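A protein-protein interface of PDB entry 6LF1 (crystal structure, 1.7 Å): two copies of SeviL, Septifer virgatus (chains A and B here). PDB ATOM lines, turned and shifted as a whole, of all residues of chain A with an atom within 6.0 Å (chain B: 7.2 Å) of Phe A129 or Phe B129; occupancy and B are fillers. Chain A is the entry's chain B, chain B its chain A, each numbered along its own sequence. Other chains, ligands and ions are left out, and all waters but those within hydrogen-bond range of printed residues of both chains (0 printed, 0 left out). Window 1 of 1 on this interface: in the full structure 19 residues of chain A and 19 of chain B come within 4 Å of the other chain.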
ATOM      1  N   LYS A  11       6.413  11.697  19.067  1.00  0.00           N
ATOM      2  CA  LYS A  11       5.268  10.994  19.634  1.00  0.00           C
ATOM      3  C   LYS A  11       4.410  10.432  18.505  1.00  0.00           C
ATOM      4  O   LYS A  11       4.056  11.157  17.570  1.00  0.00           O
ATOM      5  CB  LYS A  11       4.451  11.938  20.506  1.00  0.00           C
ATOM      6  CG  LYS A  11       5.203  12.486  21.710  1.00  0.00           C
ATOM      7  CD  LYS A  11       5.433  11.405  22.757  1.00  0.00           C
ATOM      8  CE  LYS A  11       6.023  11.995  24.036  1.00  0.00           C
ATOM      9  NZ  LYS A  11       7.288  12.736  23.760  1.00  0.00           N
ATOM     10  N   CYS A  12       4.070   9.144  18.585  1.00  0.00           N
ATOM     11  CA  CYS A  12       3.341   8.516  17.495  1.00  0.00           C
ATOM     12  C   CYS A  12       2.504   7.351  18.000  1.00  0.00           C
ATOM     13  O   CYS A  12       2.753   6.789  19.068  1.00  0.00           O
ATOM     14  CB  CYS A  12       4.295   8.022  16.401  1.00  0.00           C
ATOM     15  SG  CYS A  12       5.465   6.763  16.949  1.00  0.00           S
ATOM     16  N   TYR A  13       1.497   6.999  17.200  1.00  0.00           N
ATOM     17  CA  TYR A  13       0.813   5.718  17.338  1.00  0.00           C
ATOM     18  C   TYR A  13       1.466   4.712  16.393  1.00  0.00           C
ATOM     19  O   TYR A  13       2.028   5.087  15.365  1.00  0.00           O
ATOM     20  CB  TYR A  13      -0.676   5.823  17.009  1.00  0.00           C
ATOM     21  CG  TYR A  13      -1.491   6.714  17.918  1.00  0.00           C
ATOM     22  CD1 TYR A  13      -2.094   6.203  19.074  1.00  0.00           C
ATOM     23  CD2 TYR A  13      -1.699   8.048  17.599  1.00  0.00           C
ATOM     24  CE1 TYR A  13      -2.860   7.013  19.894  1.00  0.00           C
ATOM     25  CE2 TYR A  13      -2.464   8.868  18.419  1.00  0.00           C
ATOM     26  CZ  TYR A  13      -3.034   8.347  19.562  1.00  0.00           C
ATOM     27  OH  TYR A  13      -3.794   9.176  20.361  1.00  0.00           O
ATOM     28  N   ILE A  14       1.395   3.431  16.750  1.00  0.00           N
ATOM     29  CA  ILE A  14       2.022   2.354  15.989  1.00  0.00           C
ATOM     30  C   ILE A  14       0.910   1.362  15.693  1.00  0.00           C
ATOM     31  O   ILE A  14       0.528   0.566  16.560  1.00  0.00           O
ATOM     32  CB  ILE A  14       3.185   1.698  16.745  1.00  0.00           C
ATOM     33  CG1 ILE A  14       4.258   2.749  17.069  1.00  0.00           C
ATOM     34  CG2 ILE A  14       3.785   0.549  15.931  1.00  0.00           C
ATOM     35  CD1 ILE A  14       5.399   2.218  17.929  1.00  0.00           C
ATOM     36  N   GLN A  15       0.354   1.438  14.485  1.00  0.00           N
ATOM     37  CA  GLN A  15      -0.882   0.756  14.151  1.00  0.00           C
ATOM     38  C   GLN A  15      -0.634  -0.323  13.099  1.00  0.00           C
ATOM     39  O   GLN A  15       0.119  -0.112  12.147  1.00  0.00           O
ATOM     40  CB  GLN A  15      -1.905   1.768  13.637  1.00  0.00           C
ATOM     41  CG  GLN A  15      -3.278   1.188  13.404  1.00  0.00           C
ATOM     42  CD  GLN A  15      -4.351   2.255  13.407  1.00  0.00           C
ATOM     43  OE1 GLN A  15      -4.598   2.884  14.432  1.00  0.00           O
ATOM     44  NE2 GLN A  15      -5.014   2.449  12.266  1.00  0.00           N
ATOM     45  N   ARG A  22      -3.395  -1.161  17.720  1.00  0.00           N
ATOM     46  CA  ARG A  22      -2.260  -0.326  18.071  1.00  0.00           C
ATOM     47  C   ARG A  22      -1.471  -0.938  19.220  1.00  0.00           C
ATOM     48  O   ARG A  22      -2.040  -1.470  20.178  1.00  0.00           O
ATOM     49  CB  ARG A  22      -2.704   1.104  18.425  1.00  0.00           C
ATOM     50  CG  ARG A  22      -2.989   1.931  17.164  1.00  0.00           C
ATOM     51  CD  ARG A  22      -3.714   3.247  17.423  1.00  0.00           C
ATOM     52  NE  ARG A  22      -4.809   3.031  18.342  1.00  0.00           N
ATOM     53  CZ  ARG A  22      -5.971   2.481  18.026  1.00  0.00           C
ATOM     54  NH1 ARG A  22      -6.856   2.273  18.985  1.00  0.00           N
ATOM     55  NH2 ARG A  22      -6.247   2.145  16.766  1.00  0.00           N
ATOM     56  N   MET A  39      -8.762   4.688  21.124  1.00  0.00           N
ATOM     57  CA  MET A  39      -7.390   5.215  21.072  1.00  0.00           C
ATOM     58  C   MET A  39      -6.983   5.810  22.423  1.00  0.00           C
ATOM     59  O   MET A  39      -6.987   7.025  22.636  1.00  0.00           O
ATOM     60  CB  MET A  39      -7.271   6.249  19.964  1.00  0.00           C
ATOM     61  CG  MET A  39      -7.640   5.667  18.592  1.00  0.00           C
ATOM     62  SD  MET A  39      -7.378   6.847  17.267  1.00  0.00           S
ATOM     63  CE  MET A  39      -5.582   7.006  17.296  1.00  0.00           C
ATOM     64  N   ILE A 127       2.044   1.106  10.468  1.00  0.00           N
ATOM     65  CA  ILE A 127       2.114   2.512  10.104  1.00  0.00           C
ATOM     66  C   ILE A 127       2.321   3.313  11.381  1.00  0.00           C
ATOM     67  O   ILE A 127       1.633   3.087  12.384  1.00  0.00           O
ATOM     68  CB  ILE A 127       0.864   2.981   9.333  1.00  0.00           C
ATOM     69  CG1 ILE A 127       0.988   4.451   8.922  1.00  0.00           C
ATOM     70  CG2 ILE A 127      -0.412   2.730  10.119  1.00  0.00           C
ATOM     71  CD1 ILE A 127       0.060   4.852   7.788  1.00  0.00           C
ATOM     72  N   LEU A 128       3.310   4.190  11.363  1.00  0.00           N
ATOM     73  CA  LEU A 128       3.631   5.031  12.510  1.00  0.00           C
ATOM     74  C   LEU A 128       3.198   6.449  12.182  1.00  0.00           C
ATOM     75  O   LEU A 128       3.705   7.041  11.224  1.00  0.00           O
ATOM     76  CB  LEU A 128       5.125   4.974  12.834  1.00  0.00           C
ATOM     77  CG  LEU A 128       5.677   3.583  13.203  1.00  0.00           C
ATOM     78  CD1 LEU A 128       6.172   2.809  11.966  1.00  0.00           C
ATOM     79  CD2 LEU A 128       6.768   3.674  14.271  1.00  0.00           C
ATOM     80  N   PHE A 129       2.242   6.983  12.943  1.00  0.00           N
ATOM     81  CA  PHE A 129       1.699   8.296  12.628  1.00  0.00           C
ATOM     82  C   PHE A 129       1.687   9.202  13.851  1.00  0.00           C
ATOM     83  O   PHE A 129       1.539   8.739  14.984  1.00  0.00           O
ATOM     84  CB  PHE A 129       0.281   8.188  11.996  1.00  0.00           C
ATOM     85  CG  PHE A 129      -0.783   7.501  12.848  1.00  0.00           C
ATOM     86  CD1 PHE A 129      -1.660   8.252  13.633  1.00  0.00           C
ATOM     87  CD2 PHE A 129      -0.986   6.125  12.760  1.00  0.00           C
ATOM     88  CE1 PHE A 129      -2.681   7.636  14.363  1.00  0.00           C
ATOM     89  CE2 PHE A 129      -2.010   5.494  13.491  1.00  0.00           C
ATOM     90  CZ  PHE A 129      -2.855   6.253  14.292  1.00  0.00           C
ATOM     91  N   LYS A 130       1.834  10.507  13.594  1.00  0.00           N
ATOM     92  CA  LYS A 130       1.967  11.503  14.655  1.00  0.00           C
ATOM     93  C   LYS A 130       0.775  11.476  15.601  1.00  0.00           C
ATOM     94  O   LYS A 130      -0.379  11.465  15.168  1.00  0.00           O
ATOM     95  CB  LYS A 130       2.094  12.898  14.050  1.00  0.00           C
ATOM     96  CG  LYS A 130       3.477  13.253  13.592  1.00  0.00           C
ATOM     97  CD  LYS A 130       4.414  13.361  14.783  1.00  0.00           C
ATOM     98  CE  LYS A 130       5.611  14.174  14.398  1.00  0.00           C
ATOM     99  NZ  LYS A 130       6.077  13.840  13.018  1.00  0.00           N
ATOM    100  N   ALA A 131       1.056  11.487  16.901  1.00  0.00           N
ATOM    101  CA  ALA A 131      -0.035  11.456  17.869  1.00  0.00           C
ATOM    102  C   ALA A 131      -0.747  12.803  17.958  1.00  0.00           C
ATOM    103  O   ALA A 131      -1.976  12.856  18.109  1.00  0.00           O
ATOM    104  CB  ALA A 131       0.496  11.025  19.234  1.00  0.00           C
ATOM    105  N   THR B   8      -2.973  18.153   8.916  1.00  0.00           N
ATOM    106  CA  THR B   8      -2.419  17.558   7.702  1.00  0.00           C
ATOM    107  C   THR B   8      -3.110  18.099   6.452  1.00  0.00           C
ATOM    108  O   THR B   8      -4.329  18.290   6.431  1.00  0.00           O
ATOM    109  CB  THR B   8      -2.567  16.028   7.752  1.00  0.00           C
ATOM    110  OG1 THR B   8      -1.916  15.508   8.921  1.00  0.00           O
ATOM    111  CG2 THR B   8      -1.969  15.371   6.501  1.00  0.00           C
ATOM    112  N   GLY B  10      -3.094  17.115   2.262  1.00  0.00           N
ATOM    113  CA  GLY B  10      -2.691  16.056   1.360  1.00  0.00           C
ATOM    114  C   GLY B  10      -3.371  14.745   1.722  1.00  0.00           C
ATOM    115  O   GLY B  10      -4.459  14.738   2.312  1.00  0.00           O
ATOM    116  N   LYS B  11      -2.695  13.640   1.402  1.00  0.00           N
ATOM    117  CA  LYS B  11      -3.266  12.313   1.600  1.00  0.00           C
ATOM    118  C   LYS B  11      -3.209  11.907   3.071  1.00  0.00           C
ATOM    119  O   LYS B  11      -2.146  11.958   3.698  1.00  0.00           O
ATOM    120  CB  LYS B  11      -2.525  11.277   0.750  1.00  0.00           C
ATOM    121  CG  LYS B  11      -2.529  11.551  -0.757  1.00  0.00           C
ATOM    122  CD  LYS B  11      -3.807  11.052  -1.422  1.00  0.00           C
ATOM    123  CE  LYS B  11      -3.748  11.231  -2.933  1.00  0.00           C
ATOM    124  NZ  LYS B  11      -3.554  12.665  -3.281  1.00  0.00           N
ATOM    125  N   CYS B  12      -4.345  11.451   3.602  1.00  0.00           N
ATOM    126  CA  CYS B  12      -4.455  11.170   5.031  1.00  0.00           C
ATOM    127  C   CYS B  12      -5.517  10.107   5.298  1.00  0.00           C
ATOM    128  O   CYS B  12      -6.429   9.886   4.503  1.00  0.00           O
ATOM    129  CB  CYS B  12      -4.807  12.437   5.813  1.00  0.00           C
ATOM    130  SG  CYS B  12      -6.389  13.155   5.297  1.00  0.00           S
ATOM    131  N   TYR B  13      -5.388   9.450   6.445  1.00  0.00           N
ATOM    132  CA  TYR B  13      -6.481   8.652   6.986  1.00  0.00           C
ATOM    133  C   TYR B  13      -7.291   9.535   7.923  1.00  0.00           C
ATOM    134  O   TYR B  13      -6.779  10.509   8.465  1.00  0.00           O
ATOM    135  CB  TYR B  13      -5.963   7.434   7.753  1.00  0.00           C
ATOM    136  CG  TYR B  13      -5.208   6.417   6.910  1.00  0.00           C
ATOM    137  CD1 TYR B  13      -3.845   6.549   6.685  1.00  0.00           C
ATOM    138  CD2 TYR B  13      -5.859   5.305   6.396  1.00  0.00           C
ATOM    139  CE1 TYR B  13      -3.148   5.611   5.938  1.00  0.00           C
ATOM    140  CE2 TYR B  13      -5.182   4.365   5.630  1.00  0.00           C
ATOM    141  CZ  TYR B  13      -3.828   4.521   5.412  1.00  0.00           C
ATOM    142  OH  TYR B  13      -3.150   3.582   4.669  1.00  0.00           O
ATOM    143  N   ILE B  14      -8.558   9.198   8.105  1.00  0.00           N
ATOM    144  CA  ILE B  14      -9.451   9.954   8.981  1.00  0.00           C
ATOM    145  C   ILE B  14     -10.049   8.951   9.963  1.00  0.00           C
ATOM    146  O   ILE B  14     -10.973   8.209   9.624  1.00  0.00           O
ATOM    147  CB  ILE B  14     -10.530  10.708   8.194  1.00  0.00           C
ATOM    148  CG1 ILE B  14      -9.854  11.682   7.227  1.00  0.00           C
ATOM    149  CG2 ILE B  14     -11.456  11.460   9.146  1.00  0.00           C
ATOM    150  CD1 ILE B  14     -10.800  12.485   6.358  1.00  0.00           C
ATOM    151  N   GLN B  15      -9.525   8.931  11.193  1.00  0.00           N
ATOM    152  CA  GLN B  15      -9.779   7.845  12.127  1.00  0.00           C
ATOM    153  C   GLN B  15     -10.412   8.376  13.408  1.00  0.00           C
ATOM    154  O   GLN B  15     -10.049   9.451  13.897  1.00  0.00           O
ATOM    155  CB  GLN B  15      -8.475   7.113  12.424  1.00  0.00           C
ATOM    156  CG  GLN B  15      -8.619   5.965  13.407  1.00  0.00           C
ATOM    157  CD  GLN B  15      -7.390   5.077  13.397  1.00  0.00           C
ATOM    158  OE1 GLN B  15      -7.000   4.567  12.350  1.00  0.00           O
ATOM    159  NE2 GLN B  15      -6.759   4.912  14.557  1.00  0.00           N
ATOM    160  N   ASN B  16     -11.355   7.609  13.949  1.00  0.00           N
ATOM    161  CA  ASN B  16     -12.158   8.034  15.086  1.00  0.00           C
ATOM    162  C   ASN B  16     -11.526   7.576  16.394  1.00  0.00           C
ATOM    163  O   ASN B  16     -11.107   6.423  16.521  1.00  0.00           O
ATOM    164  CB  ASN B  16     -13.575   7.473  14.981  1.00  0.00           C
ATOM    165  CG  ASN B  16     -14.564   8.238  15.850  1.00  0.00           C
ATOM    166  OD1 ASN B  16     -14.633   8.034  17.063  1.00  0.00           O
ATOM    167  ND2 ASN B  16     -15.325   9.131  15.230  1.00  0.00           N
ATOM    168  N   GLY B  20     -11.229   3.563  16.840  1.00  0.00           N
ATOM    169  CA  GLY B  20     -10.157   3.369  15.896  1.00  0.00           C
ATOM    170  C   GLY B  20     -10.604   3.160  14.470  1.00  0.00           C
ATOM    171  O   GLY B  20      -9.772   2.797  13.628  1.00  0.00           O
ATOM    172  N   ARG B  22     -11.901   3.867  10.605  1.00  0.00           N
ATOM    173  CA  ARG B  22     -11.489   4.776   9.542  1.00  0.00           C
ATOM    174  C   ARG B  22     -12.612   5.018   8.533  1.00  0.00           C
ATOM    175  O   ARG B  22     -13.252   4.072   8.060  1.00  0.00           O
ATOM    176  CB  ARG B  22     -10.249   4.228   8.844  1.00  0.00           C
ATOM    177  CG  ARG B  22      -8.967   4.532   9.616  1.00  0.00           C
ATOM    178  CD  ARG B  22      -8.032   3.316   9.674  1.00  0.00           C
ATOM    179  NE  ARG B  22      -8.419   2.386  10.729  1.00  0.00           N
ATOM    180  CZ  ARG B  22      -8.751   1.111  10.536  1.00  0.00           C
ATOM    181  NH1 ARG B  22      -8.731   0.594   9.316  1.00  0.00           N
ATOM    182  NH2 ARG B  22      -9.086   0.341  11.576  1.00  0.00           N
ATOM    183  N   MET B  39      -6.609  -1.925   7.248  1.00  0.00           N
ATOM    184  CA  MET B  39      -6.383  -0.612   6.634  1.00  0.00           C
ATOM    185  C   MET B  39      -6.263  -0.759   5.121  1.00  0.00           C
ATOM    186  O   MET B  39      -5.185  -1.039   4.595  1.00  0.00           O
ATOM    187  CB  MET B  39      -5.132   0.039   7.209  1.00  0.00           C
ATOM    188  CG  MET B  39      -5.205   0.222   8.735  1.00  0.00           C
ATOM    189  SD  MET B  39      -3.753   1.071   9.392  1.00  0.00           S
ATOM    190  CE  MET B  39      -3.990   2.715   8.714  1.00  0.00           C
ATOM    191  N   TRP B  45      -7.723   9.642   2.095  1.00  0.00           N
ATOM    192  CA  TRP B  45      -8.461  10.805   1.629  1.00  0.00           C
ATOM    193  C   TRP B  45      -7.496  11.917   1.250  1.00  0.00           C
ATOM    194  O   TRP B  45      -6.342  11.937   1.677  1.00  0.00           O
ATOM    195  CB  TRP B  45      -9.424  11.303   2.717  1.00  0.00           C
ATOM    196  CG  TRP B  45     -10.467  10.307   3.106  1.00  0.00           C
ATOM    197  CD1 TRP B  45     -10.315   9.225   3.948  1.00  0.00           C
ATOM    198  CD2 TRP B  45     -11.834  10.288   2.677  1.00  0.00           C
ATOM    199  NE1 TRP B  45     -11.504   8.546   4.057  1.00  0.00           N
ATOM    200  CE2 TRP B  45     -12.451   9.176   3.288  1.00  0.00           C
ATOM    201  CE3 TRP B  45     -12.594  11.101   1.820  1.00  0.00           C
ATOM    202  CZ2 TRP B  45     -13.791   8.857   3.082  1.00  0.00           C
ATOM    203  CZ3 TRP B  45     -13.930  10.788   1.618  1.00  0.00           C
ATOM    204  CH2 TRP B  45     -14.521   9.676   2.250  1.00  0.00           C
ATOM    205  N   GLY B  94      -4.443  16.725  19.013  1.00  0.00           N
ATOM    206  CA  GLY B  94      -4.333  15.922  17.817  1.00  0.00           C
ATOM    207  C   GLY B  94      -5.659  15.487  17.229  1.00  0.00           C
ATOM    208  O   GLY B  94      -5.685  15.026  16.084  1.00  0.00           O
ATOM    209  N   PHE B  95      -6.751  15.624  17.973  1.00  0.00           N
ATOM    210  CA  PHE B  95      -8.074  15.240  17.508  1.00  0.00           C
ATOM    211  C   PHE B  95      -8.921  16.471  17.219  1.00  0.00           C
ATOM    212  O   PHE B  95      -8.769  17.516  17.859  1.00  0.00           O
ATOM    213  CB  PHE B  95      -8.774  14.351  18.532  1.00  0.00           C
ATOM    214  CG  PHE B  95      -8.176  12.978  18.635  1.00  0.00           C
ATOM    215  CD1 PHE B  95      -7.098  12.742  19.475  1.00  0.00           C
ATOM    216  CD2 PHE B  95      -8.675  11.928  17.868  1.00  0.00           C
ATOM    217  CE1 PHE B  95      -6.531  11.481  19.561  1.00  0.00           C
ATOM    218  CE2 PHE B  95      -8.107  10.656  17.954  1.00  0.00           C
ATOM    219  CZ  PHE B  95      -7.039  10.442  18.804  1.00  0.00           C
ATOM    220  N   TRP B 126     -11.950  13.021  15.565  1.00  0.00           N
ATOM    221  CA  TRP B 126     -11.191  12.423  14.468  1.00  0.00           C
ATOM    222  C   TRP B 126      -9.727  12.847  14.502  1.00  0.00           C
ATOM    223  O   TRP B 126      -9.411  14.008  14.776  1.00  0.00           O
ATOM    224  CB  TRP B 126     -11.791  12.817  13.106  1.00  0.00           C
ATOM    225  CG  TRP B 126     -13.263  12.482  12.975  1.00  0.00           C
ATOM    226  CD1 TRP B 126     -14.322  13.286  13.312  1.00  0.00           C
ATOM    227  CD2 TRP B 126     -13.830  11.258  12.481  1.00  0.00           C
ATOM    228  NE1 TRP B 126     -15.512  12.635  13.063  1.00  0.00           N
ATOM    229  CE2 TRP B 126     -15.238  11.392  12.547  1.00  0.00           C
ATOM    230  CE3 TRP B 126     -13.287  10.066  11.977  1.00  0.00           C
ATOM    231  CZ2 TRP B 126     -16.110  10.375  12.137  1.00  0.00           C
ATOM    232  CZ3 TRP B 126     -14.162   9.057  11.566  1.00  0.00           C
ATOM    233  CH2 TRP B 126     -15.552   9.226  11.644  1.00  0.00           C
ATOM    234  N   ILE B 127      -8.833  11.909  14.191  1.00  0.00           N
ATOM    235  CA  ILE B 127      -7.433  12.227  13.932  1.00  0.00           C
ATOM    236  C   ILE B 127      -7.177  12.029  12.446  1.00  0.00           C
ATOM    237  O   ILE B 127      -7.515  10.981  11.875  1.00  0.00           O
ATOM    238  CB  ILE B 127      -6.464  11.397  14.799  1.00  0.00           C
ATOM    239  CG1 ILE B 127      -5.014  11.815  14.535  1.00  0.00           C
ATOM    240  CG2 ILE B 127      -6.642   9.881  14.583  1.00  0.00           C
ATOM    241  CD1 ILE B 127      -4.027  11.291  15.579  1.00  0.00           C
ATOM    242  N   LEU B 128      -6.608  13.046  11.819  1.00  0.00           N
ATOM    243  CA  LEU B 128      -6.325  13.047  10.388  1.00  0.00           C
ATOM    244  C   LEU B 128      -4.817  12.929  10.249  1.00  0.00           C
ATOM    245  O   LEU B 128      -4.093  13.904  10.468  1.00  0.00           O
ATOM    246  CB  LEU B 128      -6.857  14.311   9.722  1.00  0.00           C
ATOM    247  CG  LEU B 128      -8.381  14.461   9.713  1.00  0.00           C
ATOM    248  CD1 LEU B 128      -8.908  15.076  11.005  1.00  0.00           C
ATOM    249  CD2 LEU B 128      -8.823  15.276   8.507  1.00  0.00           C
ATOM    250  N   PHE B 129      -4.334  11.741   9.896  1.00  0.00           N
ATOM    251  CA  PHE B 129      -2.899  11.523   9.898  1.00  0.00           C
ATOM    252  C   PHE B 129      -2.391  11.191   8.506  1.00  0.00           C
ATOM    253  O   PHE B 129      -3.088  10.561   7.707  1.00  0.00           O
ATOM    254  CB  PHE B 129      -2.480  10.432  10.908  1.00  0.00           C
ATOM    255  CG  PHE B 129      -3.120   9.065  10.715  1.00  0.00           C
ATOM    256  CD1 PHE B 129      -4.298   8.726  11.377  1.00  0.00           C
ATOM    257  CD2 PHE B 129      -2.477   8.080   9.972  1.00  0.00           C
ATOM    258  CE1 PHE B 129      -4.844   7.447  11.253  1.00  0.00           C
ATOM    259  CE2 PHE B 129      -3.014   6.803   9.851  1.00  0.00           C
ATOM    260  CZ  PHE B 129      -4.193   6.481  10.496  1.00  0.00           C
ATOM    261  N   LYS B 130      -1.153  11.618   8.239  1.00  0.00           N
ATOM    262  CA  LYS B 130      -0.554  11.429   6.923  1.00  0.00           C
ATOM    263  C   LYS B 130      -0.575   9.962   6.516  1.00  0.00           C
ATOM    264  O   LYS B 130      -0.227   9.069   7.297  1.00  0.00           O
ATOM    265  CB  LYS B 130       0.892  11.935   6.913  1.00  0.00           C
ATOM    266  CG  LYS B 130       1.042  13.411   7.202  1.00  0.00           C
ATOM    267  CD  LYS B 130       2.517  13.826   7.200  1.00  0.00           C
ATOM    268  CE  LYS B 130       2.658  15.293   7.564  1.00  0.00           C
ATOM    269  NZ  LYS B 130       4.085  15.727   7.572  1.00  0.00           N
ATOM    270  N   ALA B 131      -0.970   9.716   5.274  1.00  0.00           N
ATOM    271  CA  ALA B 131      -0.985   8.340   4.805  1.00  0.00           C
ATOM    272  C   ALA B 131       0.420   7.846   4.491  1.00  0.00           C
ATOM    273  O   ALA B 131       0.689   6.646   4.603  1.00  0.00           O
ATOM    274  CB  ALA B 131      -1.893   8.212   3.586  1.00  0.00           C
ATOM    275  N   TYR B 132       1.325   8.750   4.128  1.00  0.00           N
ATOM    276  CA  TYR B 132       2.663   8.359   3.695  1.00  0.00           C
ATOM    277  C   TYR B 132       3.740   9.114   4.477  1.00  0.00           C
ATOM    278  O   TYR B 132       4.903   9.137   4.081  1.00  0.00           O
ATOM    279  CB  TYR B 132       2.825   8.613   2.196  1.00  0.00           C
ATOM    280  CG  TYR B 132       1.702   8.062   1.341  1.00  0.00           C
ATOM    281  CD1 TYR B 132       1.310   6.733   1.436  1.00  0.00           C
ATOM    282  CD2 TYR B 132       1.013   8.883   0.460  1.00  0.00           C
ATOM    283  CE1 TYR B 132       0.279   6.234   0.654  1.00  0.00           C
ATOM    284  CE2 TYR B 132      -0.018   8.397  -0.318  1.00  0.00           C
ATOM    285  CZ  TYR B 132      -0.378   7.070  -0.219  1.00  0.00           C
ATOM    286  OH  TYR B 132      -1.407   6.589  -0.993  1.00  0.00           O
ATOM    287  OXT TYR B 132       3.480   9.725   5.517  1.00  0.00           O
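Of chain B, only Phe B129 (3.4 Å) comes within 4 Å of Phe A129.
Phe B129 touches one residue of chain A.
Printed residues of chain B within 4 Å of Ile A127: Tyr B13 (3.8 Å), Met B39 (3.8 Å) and Ala B131 (3.7 Å).
Printed residues of chain B within 4 Å of Arg A22: Gln B15 (3.6 Å).
Printed residues of chain A within 4 Å of Ile B127: Lys A130 (3.7 Å) and Ala A131 (3.6 Å).
Printed residues of chain B within 4 Å of Ala A131: Gly B94 and Ile B127.
The nearest residue of chain A that does not touch Phe B129 is Ile A127 (4.2 Å).
The nearest printed residue of chain B that does not touch Arg A22 is Gly B20 (4.2 Å).
Printed residues of chain B that touch a printed residue of chain A: Tyr B13, Gln B15, Asn B16, Arg B22, Met B39, Gly B94, Phe B95, Ile B127, Phe B129 and Ala B131.
Hydrophobic or aromatic side chains of chain B that line the printed part of chain A: Tyr B13, Met B39, Phe B95, Ile B127 and Phe B129.
Printed residues of chain A that touch a printed residue of chain B: Tyr A13, Gln A15, Arg A22, Met A39, Ile A127, Phe A129, Lys A130 and Ala A131.
O of Phe B129 is in hydrogen-bond range of N of Tyr B13, 2.8 Å away.
NE of Arg B22 lies within hydrogen-bond range of OE1 of Gln B15 (3.1 Å).
The backbone carbonyl oxygen of Gly B20 is in hydrogen-bond range of the guanidinium group of Arg B22, 3.2 Å away.
O of Lys A11 lies within hydrogen-bond range of N of Ala A131, 3.1 Å away.
N of Tyr A13 sits at hydrogen-bond distance from O of Phe A129 (2.8 Å).
OE1 of Gln A15 is in hydrogen-bond range of NH2 of Arg A22 (3.0 Å).
The side-chain amide oxygen of Gln B15 is in hydrogen-bond range of the side-chain amide nitrogen of Gln A15.
The side-chain amide nitrogen (NE2) of Gln B15 sits at hydrogen-bond distance from the side-chain sulfur (SD) of Met A39, at 3.4 Å.
The side-chain sulfur (SD) of Met B39 sits at hydrogen-bond distance from the side-chain amide nitrogen (NE2) of Gln A15 (3.4 Å).
Gln A15 touches Arg B22, and with the chains exchanged Arg A22 touches Gln B15.
Ile A127 touches Met B39, but with the chains exchanged Met A39 does not touch Ile B127 (4.1 Å).
Ile A127 touches Ala B131, and with the chains exchanged Ala A131 touches Ile B127.
Lys A130 touches Ile B127, but with the chains exchanged Ile A127 does not touch Lys B130 (4.3 Å).
Among the printed residues, merely in contact across the chains: Tyr A13 with Phe B95, Gln A15 with Arg B22, Arg A22 with Gln B15, Met A39 with Asn B16, Met A39 with Phe B95, Ile A127 with Tyr B13, Ile A127 with Met B39, Ile A127 with Ala B131, Phe A129 with Phe B129, Lys A130 with Ile B127, Ala A131 with Gly B94 and Ala A131 with Ile B127.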
